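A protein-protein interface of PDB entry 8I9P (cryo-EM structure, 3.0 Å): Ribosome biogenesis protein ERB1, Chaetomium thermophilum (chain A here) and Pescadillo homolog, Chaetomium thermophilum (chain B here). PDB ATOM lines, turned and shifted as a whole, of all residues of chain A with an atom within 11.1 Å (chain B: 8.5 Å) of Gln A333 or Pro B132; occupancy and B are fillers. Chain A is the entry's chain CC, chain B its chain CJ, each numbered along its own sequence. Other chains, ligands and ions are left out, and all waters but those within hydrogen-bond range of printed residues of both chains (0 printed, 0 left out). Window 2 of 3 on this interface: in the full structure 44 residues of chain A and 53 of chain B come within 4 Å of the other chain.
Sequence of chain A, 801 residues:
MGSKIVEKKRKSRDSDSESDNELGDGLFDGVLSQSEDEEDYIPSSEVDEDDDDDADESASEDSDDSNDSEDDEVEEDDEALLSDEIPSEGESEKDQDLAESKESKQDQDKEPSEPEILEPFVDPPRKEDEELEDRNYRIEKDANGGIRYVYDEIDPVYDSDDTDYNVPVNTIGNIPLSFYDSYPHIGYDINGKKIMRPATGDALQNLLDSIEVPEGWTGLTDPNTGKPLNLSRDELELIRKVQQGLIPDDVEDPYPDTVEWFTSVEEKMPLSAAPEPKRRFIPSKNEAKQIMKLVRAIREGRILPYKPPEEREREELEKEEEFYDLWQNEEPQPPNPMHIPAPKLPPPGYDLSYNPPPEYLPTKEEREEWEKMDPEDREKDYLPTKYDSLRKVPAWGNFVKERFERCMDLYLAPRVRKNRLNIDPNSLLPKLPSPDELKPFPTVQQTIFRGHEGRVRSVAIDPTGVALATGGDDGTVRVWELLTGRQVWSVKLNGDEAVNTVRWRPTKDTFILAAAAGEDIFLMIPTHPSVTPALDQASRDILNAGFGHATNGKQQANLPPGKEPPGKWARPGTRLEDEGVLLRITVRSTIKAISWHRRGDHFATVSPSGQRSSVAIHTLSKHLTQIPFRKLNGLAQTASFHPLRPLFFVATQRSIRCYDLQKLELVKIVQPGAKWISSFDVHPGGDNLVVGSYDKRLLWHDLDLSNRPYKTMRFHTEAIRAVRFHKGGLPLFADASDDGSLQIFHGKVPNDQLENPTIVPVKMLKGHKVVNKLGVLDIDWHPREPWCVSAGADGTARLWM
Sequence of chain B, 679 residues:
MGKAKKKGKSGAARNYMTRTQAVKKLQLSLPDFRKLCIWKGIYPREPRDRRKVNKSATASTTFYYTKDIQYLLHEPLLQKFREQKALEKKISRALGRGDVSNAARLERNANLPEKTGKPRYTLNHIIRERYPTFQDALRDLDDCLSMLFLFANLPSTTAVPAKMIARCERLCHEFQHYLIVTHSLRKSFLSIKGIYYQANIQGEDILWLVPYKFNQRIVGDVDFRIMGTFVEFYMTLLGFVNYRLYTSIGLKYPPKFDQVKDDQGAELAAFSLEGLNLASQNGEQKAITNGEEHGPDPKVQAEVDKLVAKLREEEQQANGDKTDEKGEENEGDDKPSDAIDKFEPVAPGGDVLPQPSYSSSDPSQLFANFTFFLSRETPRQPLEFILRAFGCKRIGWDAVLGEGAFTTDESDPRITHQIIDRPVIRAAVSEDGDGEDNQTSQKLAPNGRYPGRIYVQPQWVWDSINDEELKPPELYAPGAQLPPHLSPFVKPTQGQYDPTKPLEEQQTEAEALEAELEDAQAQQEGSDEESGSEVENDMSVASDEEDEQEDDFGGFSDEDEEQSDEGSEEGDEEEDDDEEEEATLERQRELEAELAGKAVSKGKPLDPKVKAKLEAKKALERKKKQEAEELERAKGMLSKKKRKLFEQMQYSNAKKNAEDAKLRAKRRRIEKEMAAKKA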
ATOM      1  N   LEU A 326       6.720  -5.399 -35.697  1.00  0.00           N
ATOM      2  CA  LEU A 326       7.999  -4.860 -35.245  1.00  0.00           C
ATOM      3  C   LEU A 326       8.954  -5.983 -34.856  1.00  0.00           C
ATOM      4  O   LEU A 326      10.163  -5.901 -35.106  1.00  0.00           O
ATOM      5  CB  LEU A 326       7.771  -3.897 -34.079  1.00  0.00           C
ATOM      6  CG  LEU A 326       8.979  -3.179 -33.478  1.00  0.00           C
ATOM      7  CD1 LEU A 326       9.851  -2.567 -34.567  1.00  0.00           C
ATOM      8  CD2 LEU A 326       8.530  -2.114 -32.490  1.00  0.00           C
ATOM      9  N   TRP A 327       8.428  -7.043 -34.246  1.00  0.00           N
ATOM     10  CA  TRP A 327       9.221  -8.219 -33.886  1.00  0.00           C
ATOM     11  C   TRP A 327       9.076  -9.302 -34.955  1.00  0.00           C
ATOM     12  O   TRP A 327       8.550 -10.390 -34.717  1.00  0.00           O
ATOM     13  CB  TRP A 327       8.801  -8.742 -32.514  1.00  0.00           C
ATOM     14  CG  TRP A 327       9.179  -7.885 -31.342  1.00  0.00           C
ATOM     15  CD1 TRP A 327      10.327  -7.967 -30.611  1.00  0.00           C
ATOM     16  CD2 TRP A 327       8.408  -6.827 -30.758  1.00  0.00           C
ATOM     17  NE1 TRP A 327      10.319  -7.033 -29.606  1.00  0.00           N
ATOM     18  CE2 TRP A 327       9.154  -6.315 -29.676  1.00  0.00           C
ATOM     19  CE3 TRP A 327       7.163  -6.259 -31.044  1.00  0.00           C
ATOM     20  CZ2 TRP A 327       8.698  -5.265 -28.884  1.00  0.00           C
ATOM     21  CZ3 TRP A 327       6.713  -5.216 -30.255  1.00  0.00           C
ATOM     22  CH2 TRP A 327       7.478  -4.731 -29.188  1.00  0.00           C
ATOM     23  N   GLN A 328       9.554  -8.985 -36.161  1.00  0.00           N
ATOM     24  CA  GLN A 328       9.561  -9.988 -37.224  1.00  0.00           C
ATOM     25  C   GLN A 328      10.628 -11.047 -36.980  1.00  0.00           C
ATOM     26  O   GLN A 328      10.367 -12.246 -37.134  1.00  0.00           O
ATOM     27  CB  GLN A 328       9.765  -9.324 -38.585  1.00  0.00           C
ATOM     28  CG  GLN A 328       8.497  -8.737 -39.181  1.00  0.00           C
ATOM     29  CD  GLN A 328       8.729  -8.101 -40.537  1.00  0.00           C
ATOM     30  OE1 GLN A 328       9.858  -8.038 -41.022  1.00  0.00           O
ATOM     31  NE2 GLN A 328       7.655  -7.626 -41.157  1.00  0.00           N
ATOM     32  N   ASN A 329      11.834 -10.628 -36.602  1.00  0.00           N
ATOM     33  CA  ASN A 329      12.928 -11.541 -36.277  1.00  0.00           C
ATOM     34  C   ASN A 329      13.421 -11.171 -34.882  1.00  0.00           C
ATOM     35  O   ASN A 329      14.316 -10.334 -34.733  1.00  0.00           O
ATOM     36  CB  ASN A 329      14.048 -11.456 -37.310  1.00  0.00           C
ATOM     37  CG  ASN A 329      14.938 -12.686 -37.308  1.00  0.00           C
ATOM     38  OD1 ASN A 329      14.866 -13.520 -36.405  1.00  0.00           O
ATOM     39  ND2 ASN A 329      15.785 -12.804 -38.325  1.00  0.00           N
ATOM     40  N   GLU A 330      12.839 -11.797 -33.863  1.00  0.00           N
ATOM     41  CA  GLU A 330      13.116 -11.473 -32.472  1.00  0.00           C
ATOM     42  C   GLU A 330      14.121 -12.459 -31.894  1.00  0.00           C
ATOM     43  O   GLU A 330      13.923 -13.675 -31.976  1.00  0.00           O
ATOM     44  CB  GLU A 330      11.833 -11.487 -31.639  1.00  0.00           C
ATOM     45  CG  GLU A 330      12.023 -11.009 -30.210  1.00  0.00           C
ATOM     46  CD  GLU A 330      10.747 -11.077 -29.396  1.00  0.00           C
ATOM     47  OE1 GLU A 330       9.821 -11.814 -29.799  1.00  0.00           O
ATOM     48  OE2 GLU A 330      10.666 -10.394 -28.354  1.00  0.00           O
ATOM     49  N   GLU A 331      15.192 -11.929 -31.315  1.00  0.00           N
ATOM     50  CA  GLU A 331      16.180 -12.704 -30.586  1.00  0.00           C
ATOM     51  C   GLU A 331      16.451 -12.034 -29.248  1.00  0.00           C
ATOM     52  O   GLU A 331      16.351 -10.807 -29.136  1.00  0.00           O
ATOM     53  CB  GLU A 331      17.490 -12.829 -31.378  1.00  0.00           C
ATOM     54  CG  GLU A 331      17.384 -13.689 -32.625  1.00  0.00           C
ATOM     55  CD  GLU A 331      18.728 -13.930 -33.283  1.00  0.00           C
ATOM     56  OE1 GLU A 331      19.747 -13.447 -32.747  1.00  0.00           O
ATOM     57  OE2 GLU A 331      18.765 -14.602 -34.335  1.00  0.00           O
ATOM     58  N   PRO A 332      16.766 -12.813 -28.211  1.00  0.00           N
ATOM     59  CA  PRO A 332      17.106 -12.211 -26.917  1.00  0.00           C
ATOM     60  C   PRO A 332      18.393 -11.402 -26.994  1.00  0.00           C
ATOM     61  O   PRO A 332      19.340 -11.767 -27.696  1.00  0.00           O
ATOM     62  CB  PRO A 332      17.257 -13.422 -25.988  1.00  0.00           C
ATOM     63  CG  PRO A 332      16.483 -14.512 -26.653  1.00  0.00           C
ATOM     64  CD  PRO A 332      16.650 -14.279 -28.123  1.00  0.00           C
ATOM     65  N   GLN A 333      18.418 -10.290 -26.262  1.00  0.00           N
ATOM     66  CA  GLN A 333      19.570  -9.403 -26.226  1.00  0.00           C
ATOM     67  C   GLN A 333      19.955  -9.157 -24.772  1.00  0.00           C
ATOM     68  O   GLN A 333      19.090  -8.789 -23.957  1.00  0.00           O
ATOM     69  CB  GLN A 333      19.270  -8.076 -26.936  1.00  0.00           C
ATOM     70  CG  GLN A 333      20.370  -7.035 -26.797  1.00  0.00           C
ATOM     71  CD  GLN A 333      20.102  -5.793 -27.623  1.00  0.00           C
ATOM     72  OE1 GLN A 333      19.463  -5.857 -28.673  1.00  0.00           O
ATOM     73  NE2 GLN A 333      20.592  -4.652 -27.151  1.00  0.00           N
ATOM     74  N   PRO A 334      21.217  -9.355 -24.403  1.00  0.00           N
ATOM     75  CA  PRO A 334      21.636  -9.123 -23.017  1.00  0.00           C
ATOM     76  C   PRO A 334      21.658  -7.641 -22.695  1.00  0.00           C
ATOM     77  O   PRO A 334      22.162  -6.831 -23.488  1.00  0.00           O
ATOM     78  CB  PRO A 334      23.051  -9.724 -22.965  1.00  0.00           C
ATOM     79  CG  PRO A 334      23.174 -10.567 -24.206  1.00  0.00           C
ATOM     80  CD  PRO A 334      22.310  -9.900 -25.223  1.00  0.00           C
ATOM     81  N   PRO A 335      21.116  -7.242 -21.543  1.00  0.00           N
ATOM     82  CA  PRO A 335      21.158  -5.824 -21.163  1.00  0.00           C
ATOM     83  C   PRO A 335      22.547  -5.435 -20.679  1.00  0.00           C
ATOM     84  O   PRO A 335      23.085  -6.038 -19.747  1.00  0.00           O
ATOM     85  CB  PRO A 335      20.119  -5.721 -20.038  1.00  0.00           C
ATOM     86  CG  PRO A 335      19.367  -7.031 -20.051  1.00  0.00           C
ATOM     87  CD  PRO A 335      20.318  -8.040 -20.601  1.00  0.00           C
ATOM     88  N   ASN A 336      23.129  -4.428 -21.326  1.00  0.00           N
ATOM     89  CA  ASN A 336      24.434  -3.942 -20.910  1.00  0.00           C
ATOM     90  C   ASN A 336      24.304  -3.198 -19.579  1.00  0.00           C
ATOM     91  O   ASN A 336      23.260  -2.595 -19.308  1.00  0.00           O
ATOM     92  CB  ASN A 336      25.036  -3.030 -21.982  1.00  0.00           C
ATOM     93  CG  ASN A 336      24.238  -1.764 -22.187  1.00  0.00           C
ATOM     94  OD1 ASN A 336      23.031  -1.801 -22.420  1.00  0.00           O
ATOM     95  ND2 ASN A 336      24.918  -0.626 -22.104  1.00  0.00           N
ATOM     96  N   PRO A 337      25.332  -3.237 -18.723  1.00  0.00           N
ATOM     97  CA  PRO A 337      25.163  -2.710 -17.358  1.00  0.00           C
ATOM     98  C   PRO A 337      25.048  -1.196 -17.266  1.00  0.00           C
ATOM     99  O   PRO A 337      24.624  -0.696 -16.217  1.00  0.00           O
ATOM    100  CB  PRO A 337      26.421  -3.211 -16.632  1.00  0.00           C
ATOM    101  CG  PRO A 337      27.424  -3.402 -17.715  1.00  0.00           C
ATOM    102  CD  PRO A 337      26.643  -3.887 -18.899  1.00  0.00           C
ATOM    103  N   MET A 338      25.411  -0.444 -18.308  1.00  0.00           N
ATOM    104  CA  MET A 338      25.430   1.009 -18.168  1.00  0.00           C
ATOM    105  C   MET A 338      24.030   1.615 -18.237  1.00  0.00           C
ATOM    106  O   MET A 338      23.749   2.592 -17.533  1.00  0.00           O
ATOM    107  CB  MET A 338      26.348   1.634 -19.218  1.00  0.00           C
ATOM    108  CG  MET A 338      26.577   3.121 -18.999  1.00  0.00           C
ATOM    109  SD  MET A 338      27.961   3.413 -17.877  1.00  0.00           S
ATOM    110  CE  MET A 338      28.284   5.149 -18.163  1.00  0.00           C
ATOM    111  N   HIS A 339      23.142   1.057 -19.061  1.00  0.00           N
ATOM    112  CA  HIS A 339      21.764   1.533 -19.126  1.00  0.00           C
ATOM    113  C   HIS A 339      21.041   1.220 -17.822  1.00  0.00           C
ATOM    114  O   HIS A 339      20.811   0.050 -17.494  1.00  0.00           O
ATOM    115  CB  HIS A 339      21.016   0.915 -20.307  1.00  0.00           C
ATOM    116  CG  HIS A 339      21.391   1.490 -21.638  1.00  0.00           C
ATOM    117  ND1 HIS A 339      22.604   1.250 -22.244  1.00  0.00           N
ATOM    118  CD2 HIS A 339      20.699   2.291 -22.485  1.00  0.00           C
ATOM    119  CE1 HIS A 339      22.648   1.881 -23.405  1.00  0.00           C
ATOM    120  NE2 HIS A 339      21.505   2.521 -23.574  1.00  0.00           N
ATOM    121  N   PRO A 341      17.566   1.569 -16.037  1.00  0.00           N
ATOM    122  CA  PRO A 341      16.159   1.892 -16.290  1.00  0.00           C
ATOM    123  C   PRO A 341      15.576   2.769 -15.195  1.00  0.00           C
ATOM    124  O   PRO A 341      16.009   2.733 -14.040  1.00  0.00           O
ATOM    125  CB  PRO A 341      15.480   0.518 -16.323  1.00  0.00           C
ATOM    126  CG  PRO A 341      16.360  -0.352 -15.491  1.00  0.00           C
ATOM    127  CD  PRO A 341      17.761   0.145 -15.711  1.00  0.00           C
ATOM    128  N   ILE B 126      14.723   4.014 -33.387  1.00  0.00           N
ATOM    129  CA  ILE B 126      15.088   4.447 -32.042  1.00  0.00           C
ATOM    130  C   ILE B 126      14.353   3.616 -30.993  1.00  0.00           C
ATOM    131  O   ILE B 126      14.951   3.179 -30.001  1.00  0.00           O
ATOM    132  CB  ILE B 126      14.832   5.959 -31.877  1.00  0.00           C
ATOM    133  CG1 ILE B 126      15.759   6.787 -32.773  1.00  0.00           C
ATOM    134  CG2 ILE B 126      14.971   6.381 -30.428  1.00  0.00           C
ATOM    135  CD1 ILE B 126      15.384   8.252 -32.857  1.00  0.00           C
ATOM    136  N   ILE B 127      13.061   3.355 -31.203  1.00  0.00           N
ATOM    137  CA  ILE B 127      12.329   2.532 -30.249  1.00  0.00           C
ATOM    138  C   ILE B 127      12.677   1.058 -30.403  1.00  0.00           C
ATOM    139  O   ILE B 127      12.449   0.273 -29.475  1.00  0.00           O
ATOM    140  CB  ILE B 127      10.812   2.759 -30.373  1.00  0.00           C
ATOM    141  CG1 ILE B 127      10.253   2.094 -31.633  1.00  0.00           C
ATOM    142  CG2 ILE B 127      10.520   4.244 -30.403  1.00  0.00           C
ATOM    143  CD1 ILE B 127       8.782   1.751 -31.538  1.00  0.00           C
ATOM    144  N   ARG B 128      13.223   0.653 -31.554  1.00  0.00           N
ATOM    145  CA  ARG B 128      13.774  -0.695 -31.661  1.00  0.00           C
ATOM    146  C   ARG B 128      15.063  -0.837 -30.863  1.00  0.00           C
ATOM    147  O   ARG B 128      15.273  -1.853 -30.190  1.00  0.00           O
ATOM    148  CB  ARG B 128      14.001  -1.059 -33.129  1.00  0.00           C
ATOM    149  CG  ARG B 128      14.314  -2.542 -33.435  1.00  0.00           C
ATOM    150  CD  ARG B 128      13.222  -3.563 -33.075  1.00  0.00           C
ATOM    151  NE  ARG B 128      13.135  -3.839 -31.646  1.00  0.00           N
ATOM    152  CZ  ARG B 128      12.157  -4.520 -31.067  1.00  0.00           C
ATOM    153  NH1 ARG B 128      11.178  -5.057 -31.775  1.00  0.00           N
ATOM    154  NH2 ARG B 128      12.164  -4.667 -29.746  1.00  0.00           N
ATOM    155  N   GLU B 129      15.939   0.165 -30.928  1.00  0.00           N
ATOM    156  CA  GLU B 129      17.215   0.078 -30.224  1.00  0.00           C
ATOM    157  C   GLU B 129      17.038   0.267 -28.722  1.00  0.00           C
ATOM    158  O   GLU B 129      17.750  -0.354 -27.925  1.00  0.00           O
ATOM    159  CB  GLU B 129      18.191   1.108 -30.791  1.00  0.00           C
ATOM    160  CG  GLU B 129      19.242   0.512 -31.715  1.00  0.00           C
ATOM    161  CD  GLU B 129      19.633   1.453 -32.836  1.00  0.00           C
ATOM    162  OE1 GLU B 129      19.260   2.643 -32.772  1.00  0.00           O
ATOM    163  OE2 GLU B 129      20.316   1.002 -33.780  1.00  0.00           O
ATOM    164  N   ARG B 130      16.098   1.125 -28.316  1.00  0.00           N
ATOM    165  CA  ARG B 130      15.895   1.380 -26.893  1.00  0.00           C
ATOM    166  C   ARG B 130      15.171   0.221 -26.214  1.00  0.00           C
ATOM    167  O   ARG B 130      15.547  -0.188 -25.109  1.00  0.00           O
ATOM    168  CB  ARG B 130      15.136   2.693 -26.707  1.00  0.00           C
ATOM    169  CG  ARG B 130      14.604   2.927 -25.308  1.00  0.00           C
ATOM    170  CD  ARG B 130      13.550   4.023 -25.311  1.00  0.00           C
ATOM    171  NE  ARG B 130      13.580   4.837 -24.102  1.00  0.00           N
ATOM    172  CZ  ARG B 130      14.506   5.747 -23.825  1.00  0.00           C
ATOM    173  NH1 ARG B 130      15.485   6.017 -24.672  1.00  0.00           N
ATOM    174  NH2 ARG B 130      14.441   6.408 -22.674  1.00  0.00           N
ATOM    175  N   TYR B 131      14.142  -0.331 -26.859  1.00  0.00           N
ATOM    176  CA  TYR B 131      13.439  -1.497 -26.330  1.00  0.00           C
ATOM    177  C   TYR B 131      13.806  -2.730 -27.141  1.00  0.00           C
ATOM    178  O   TYR B 131      13.313  -2.901 -28.267  1.00  0.00           O
ATOM    179  CB  TYR B 131      11.923  -1.283 -26.345  1.00  0.00           C
ATOM    180  CG  TYR B 131      11.467   0.016 -25.733  1.00  0.00           C
ATOM    181  CD1 TYR B 131      11.560   0.228 -24.363  1.00  0.00           C
ATOM    182  CD2 TYR B 131      10.932   1.025 -26.520  1.00  0.00           C
ATOM    183  CE1 TYR B 131      11.140   1.414 -23.796  1.00  0.00           C
ATOM    184  CE2 TYR B 131      10.510   2.212 -25.962  1.00  0.00           C
ATOM    185  CZ  TYR B 131      10.611   2.399 -24.601  1.00  0.00           C
ATOM    186  OH  TYR B 131      10.197   3.585 -24.047  1.00  0.00           O
ATOM    187  N   PRO B 132      14.657  -3.619 -26.622  1.00  0.00           N
ATOM    188  CA  PRO B 132      14.966  -4.850 -27.362  1.00  0.00           C
ATOM    189  C   PRO B 132      13.878  -5.905 -27.280  1.00  0.00           C
ATOM    190  O   PRO B 132      13.734  -6.690 -28.226  1.00  0.00           O
ATOM    191  CB  PRO B 132      16.261  -5.340 -26.699  1.00  0.00           C
ATOM    192  CG  PRO B 132      16.173  -4.822 -25.301  1.00  0.00           C
ATOM    193  CD  PRO B 132      15.429  -3.510 -25.372  1.00  0.00           C
ATOM    194  N   THR B 133      13.109  -5.950 -26.194  1.00  0.00           N
ATOM    195  CA  THR B 133      12.060  -6.942 -26.013  1.00  0.00           C
ATOM    196  C   THR B 133      10.789  -6.261 -25.520  1.00  0.00           C
ATOM    197  O   THR B 133      10.738  -5.041 -25.348  1.00  0.00           O
ATOM    198  CB  THR B 133      12.481  -8.050 -25.036  1.00  0.00           C
ATOM    199  OG1 THR B 133      13.057  -7.462 -23.861  1.00  0.00           O
ATOM    200  CG2 THR B 133      13.489  -8.993 -25.681  1.00  0.00           C
ATOM    201  N   PHE B 134       9.755  -7.076 -25.294  1.00  0.00           N
ATOM    202  CA  PHE B 134       8.413  -6.543 -25.091  1.00  0.00           C
ATOM    203  C   PHE B 134       8.133  -6.127 -23.649  1.00  0.00           C
ATOM    204  O   PHE B 134       7.312  -5.229 -23.428  1.00  0.00           O
ATOM    205  CB  PHE B 134       7.376  -7.574 -25.541  1.00  0.00           C
ATOM    206  CG  PHE B 134       5.989  -7.019 -25.670  1.00  0.00           C
ATOM    207  CD1 PHE B 134       5.786  -5.751 -26.191  1.00  0.00           C
ATOM    208  CD2 PHE B 134       4.891  -7.759 -25.267  1.00  0.00           C
ATOM    209  CE1 PHE B 134       4.513  -5.233 -26.312  1.00  0.00           C
ATOM    210  CE2 PHE B 134       3.614  -7.246 -25.384  1.00  0.00           C
ATOM    211  CZ  PHE B 134       3.427  -5.979 -25.907  1.00  0.00           C
ATOM    212  N   GLN B 135       8.772  -6.758 -22.659  1.00  0.00           N
ATOM    213  CA  GLN B 135       8.434  -6.439 -21.274  1.00  0.00           C
ATOM    214  C   GLN B 135       8.986  -5.076 -20.863  1.00  0.00           C
ATOM    215  O   GLN B 135       8.387  -4.385 -20.032  1.00  0.00           O
ATOM    216  CB  GLN B 135       8.904  -7.556 -20.329  1.00  0.00           C
ATOM    217  CG  GLN B 135      10.365  -7.556 -19.843  1.00  0.00           C
ATOM    218  CD  GLN B 135      11.418  -7.494 -20.940  1.00  0.00           C
ATOM    219  OE1 GLN B 135      11.155  -7.803 -22.100  1.00  0.00           O
ATOM    220  NE2 GLN B 135      12.630  -7.107 -20.563  1.00  0.00           N
ATOM    221  N   ASP B 136      10.102  -4.652 -21.463  1.00  0.00           N
ATOM    222  CA  ASP B 136      10.549  -3.274 -21.283  1.00  0.00           C
ATOM    223  C   ASP B 136       9.577  -2.292 -21.924  1.00  0.00           C
ATOM    224  O   ASP B 136       9.362  -1.190 -21.398  1.00  0.00           O
ATOM    225  CB  ASP B 136      11.950  -3.088 -21.864  1.00  0.00           C
ATOM    226  CG  ASP B 136      12.967  -4.018 -21.240  1.00  0.00           C
ATOM    227  OD1 ASP B 136      12.897  -4.240 -20.012  1.00  0.00           O
ATOM    228  OD2 ASP B 136      13.837  -4.531 -21.975  1.00  0.00           O
ATOM    229  N   ALA B 137       8.980  -2.684 -23.055  1.00  0.00           N
ATOM    230  CA  ALA B 137       7.955  -1.857 -23.679  1.00  0.00           C
ATOM    231  C   ALA B 137       6.734  -1.728 -22.781  1.00  0.00           C
ATOM    232  O   ALA B 137       6.137  -0.656 -22.703  1.00  0.00           O
ATOM    233  CB  ALA B 137       7.567  -2.428 -25.044  1.00  0.00           C
ATOM    234  N   ARG B 139       6.903  -1.961 -19.425  1.00  0.00           N
ATOM    235  CA  ARG B 139       7.376  -1.175 -18.287  1.00  0.00           C
ATOM    236  C   ARG B 139       7.356   0.317 -18.583  1.00  0.00           C
ATOM    237  O   ARG B 139       6.988   1.115 -17.713  1.00  0.00           O
ATOM    238  CB  ARG B 139       8.788  -1.606 -17.890  1.00  0.00           C
ATOM    239  CG  ARG B 139       8.866  -2.927 -17.148  1.00  0.00           C
ATOM    240  CD  ARG B 139      10.255  -3.533 -17.267  1.00  0.00           C
ATOM    241  NE  ARG B 139      10.318  -4.883 -16.721  1.00  0.00           N
ATOM    242  CZ  ARG B 139      11.302  -5.740 -16.955  1.00  0.00           C
ATOM    243  NH1 ARG B 139      12.330  -5.418 -17.724  1.00  0.00           N
ATOM    244  NH2 ARG B 139      11.253  -6.951 -16.407  1.00  0.00           N
ATOM    245  N   ARG B 244       1.469  -5.433 -31.851  1.00  0.00           N
ATOM    246  CA  ARG B 244       2.094  -6.666 -31.380  1.00  0.00           C
ATOM    247  C   ARG B 244       1.137  -7.498 -30.534  1.00  0.00           C
ATOM    248  O   ARG B 244       1.038  -8.716 -30.715  1.00  0.00           O
ATOM    249  CB  ARG B 244       3.364  -6.333 -30.594  1.00  0.00           C
ATOM    250  CG  ARG B 244       3.741  -7.349 -29.524  1.00  0.00           C
ATOM    251  CD  ARG B 244       4.476  -8.547 -30.098  1.00  0.00           C
ATOM    252  NE  ARG B 244       5.313  -9.192 -29.095  1.00  0.00           N
ATOM    253  CZ  ARG B 244       6.305 -10.027 -29.369  1.00  0.00           C
ATOM    254  NH1 ARG B 244       6.591 -10.374 -30.613  1.00  0.00           N
ATOM    255  NH2 ARG B 244       7.024 -10.531 -28.371  1.00  0.00           N
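The guanidinium group (NH2) of Arg B128 is in hydrogen-bond range of the backbone carbonyl oxygen (O) of Tyr B131 (2.6 Å).
The backbone carbonyl oxygen of Pro B132 lies within hydrogen-bond range of the guanidinium group of Arg B128 (3.0 Å).
OG1 of Thr B133 sits at hydrogen-bond distance from OE1 of Gln B135, 2.6 Å away.
Gln A333 touches one residue of chain B.
Of chain A, only Trp A327 (3.7 Å) and Gln A333 (3.8 Å) come within 4 Å of Pro B132.
No residue of chain B comes within 4 Å of Pro A334.
Printed residues of chain A within 4 Å of Arg B128: Leu A326 and Trp A327.
Of the printed residues of chain B, Trp A327 touches Arg B128 (3.0 Å), Pro B132 (3.7 Å), Thr B133 (3.99 Å), Phe B134 (3.6 Å) and Arg B244 (3.3 Å).
Printed residues of chain B within 4 Å of Leu A326: Ile B127 (3.99 Å) and Arg B128 (3.4 Å).
Printed residues of chain A within 4 Å of Thr B133: Trp A327 (3.99 Å).
Met A338 touches none of the printed residues of chain B.
The nearest residue of chain B that does not touch Gln A333 is Thr B133 (5.1 Å).
The nearest residue of chain A that does not touch Pro B132 is Glu A330 (4.8 Å).
The nearest printed residue of chain B that does not touch Glu A330 is Thr B133 (4.1 Å).
Ile B127 touches Leu A326 (CD1 to CD2, 3.99 Å).
NH1 of Arg B128 touches CG of Leu A326, at 3.4 Å.
Trp A327 touches Pro B132.
NE1 of Trp A327 touches CA of Thr B133 (3.99 Å).
CD1 of Phe B134 touches CH2 of Trp A327, at 3.6 Å.
CB of Trp A327 touches NH1 of Arg B244, at 3.3 Å.
Pro B132 touches Gln A333 (CB to OE1, 3.8 Å).
Hydrophobic or aromatic side chains of chain B that line the printed part of chain A: Ile B127, Pro B132 and Phe B134.
Printed residues of chain A that touch a printed residue of chain B: Leu A326, Trp A327, Glu A330 and Gln A333.
Hydrophobic or aromatic side chains of chain A that line the printed part of chain B: Leu A326 and Trp A327.
Among the printed residues, 9 pairs touch across the chains.
Among the printed residues, Asp or Glu carboxylates within 4 Å of a Lys or Arg side-chain nitrogen of the other chain: Glu A330 with Arg B244.
The side-chain carboxylate of Glu A330 lies within salt-bridge range of the guanidinium group of Arg B244 (3.4 Å).
The guanidinium group of Arg B128 lies close to the indole nitrogen of Trp A327 (3.0 Å).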
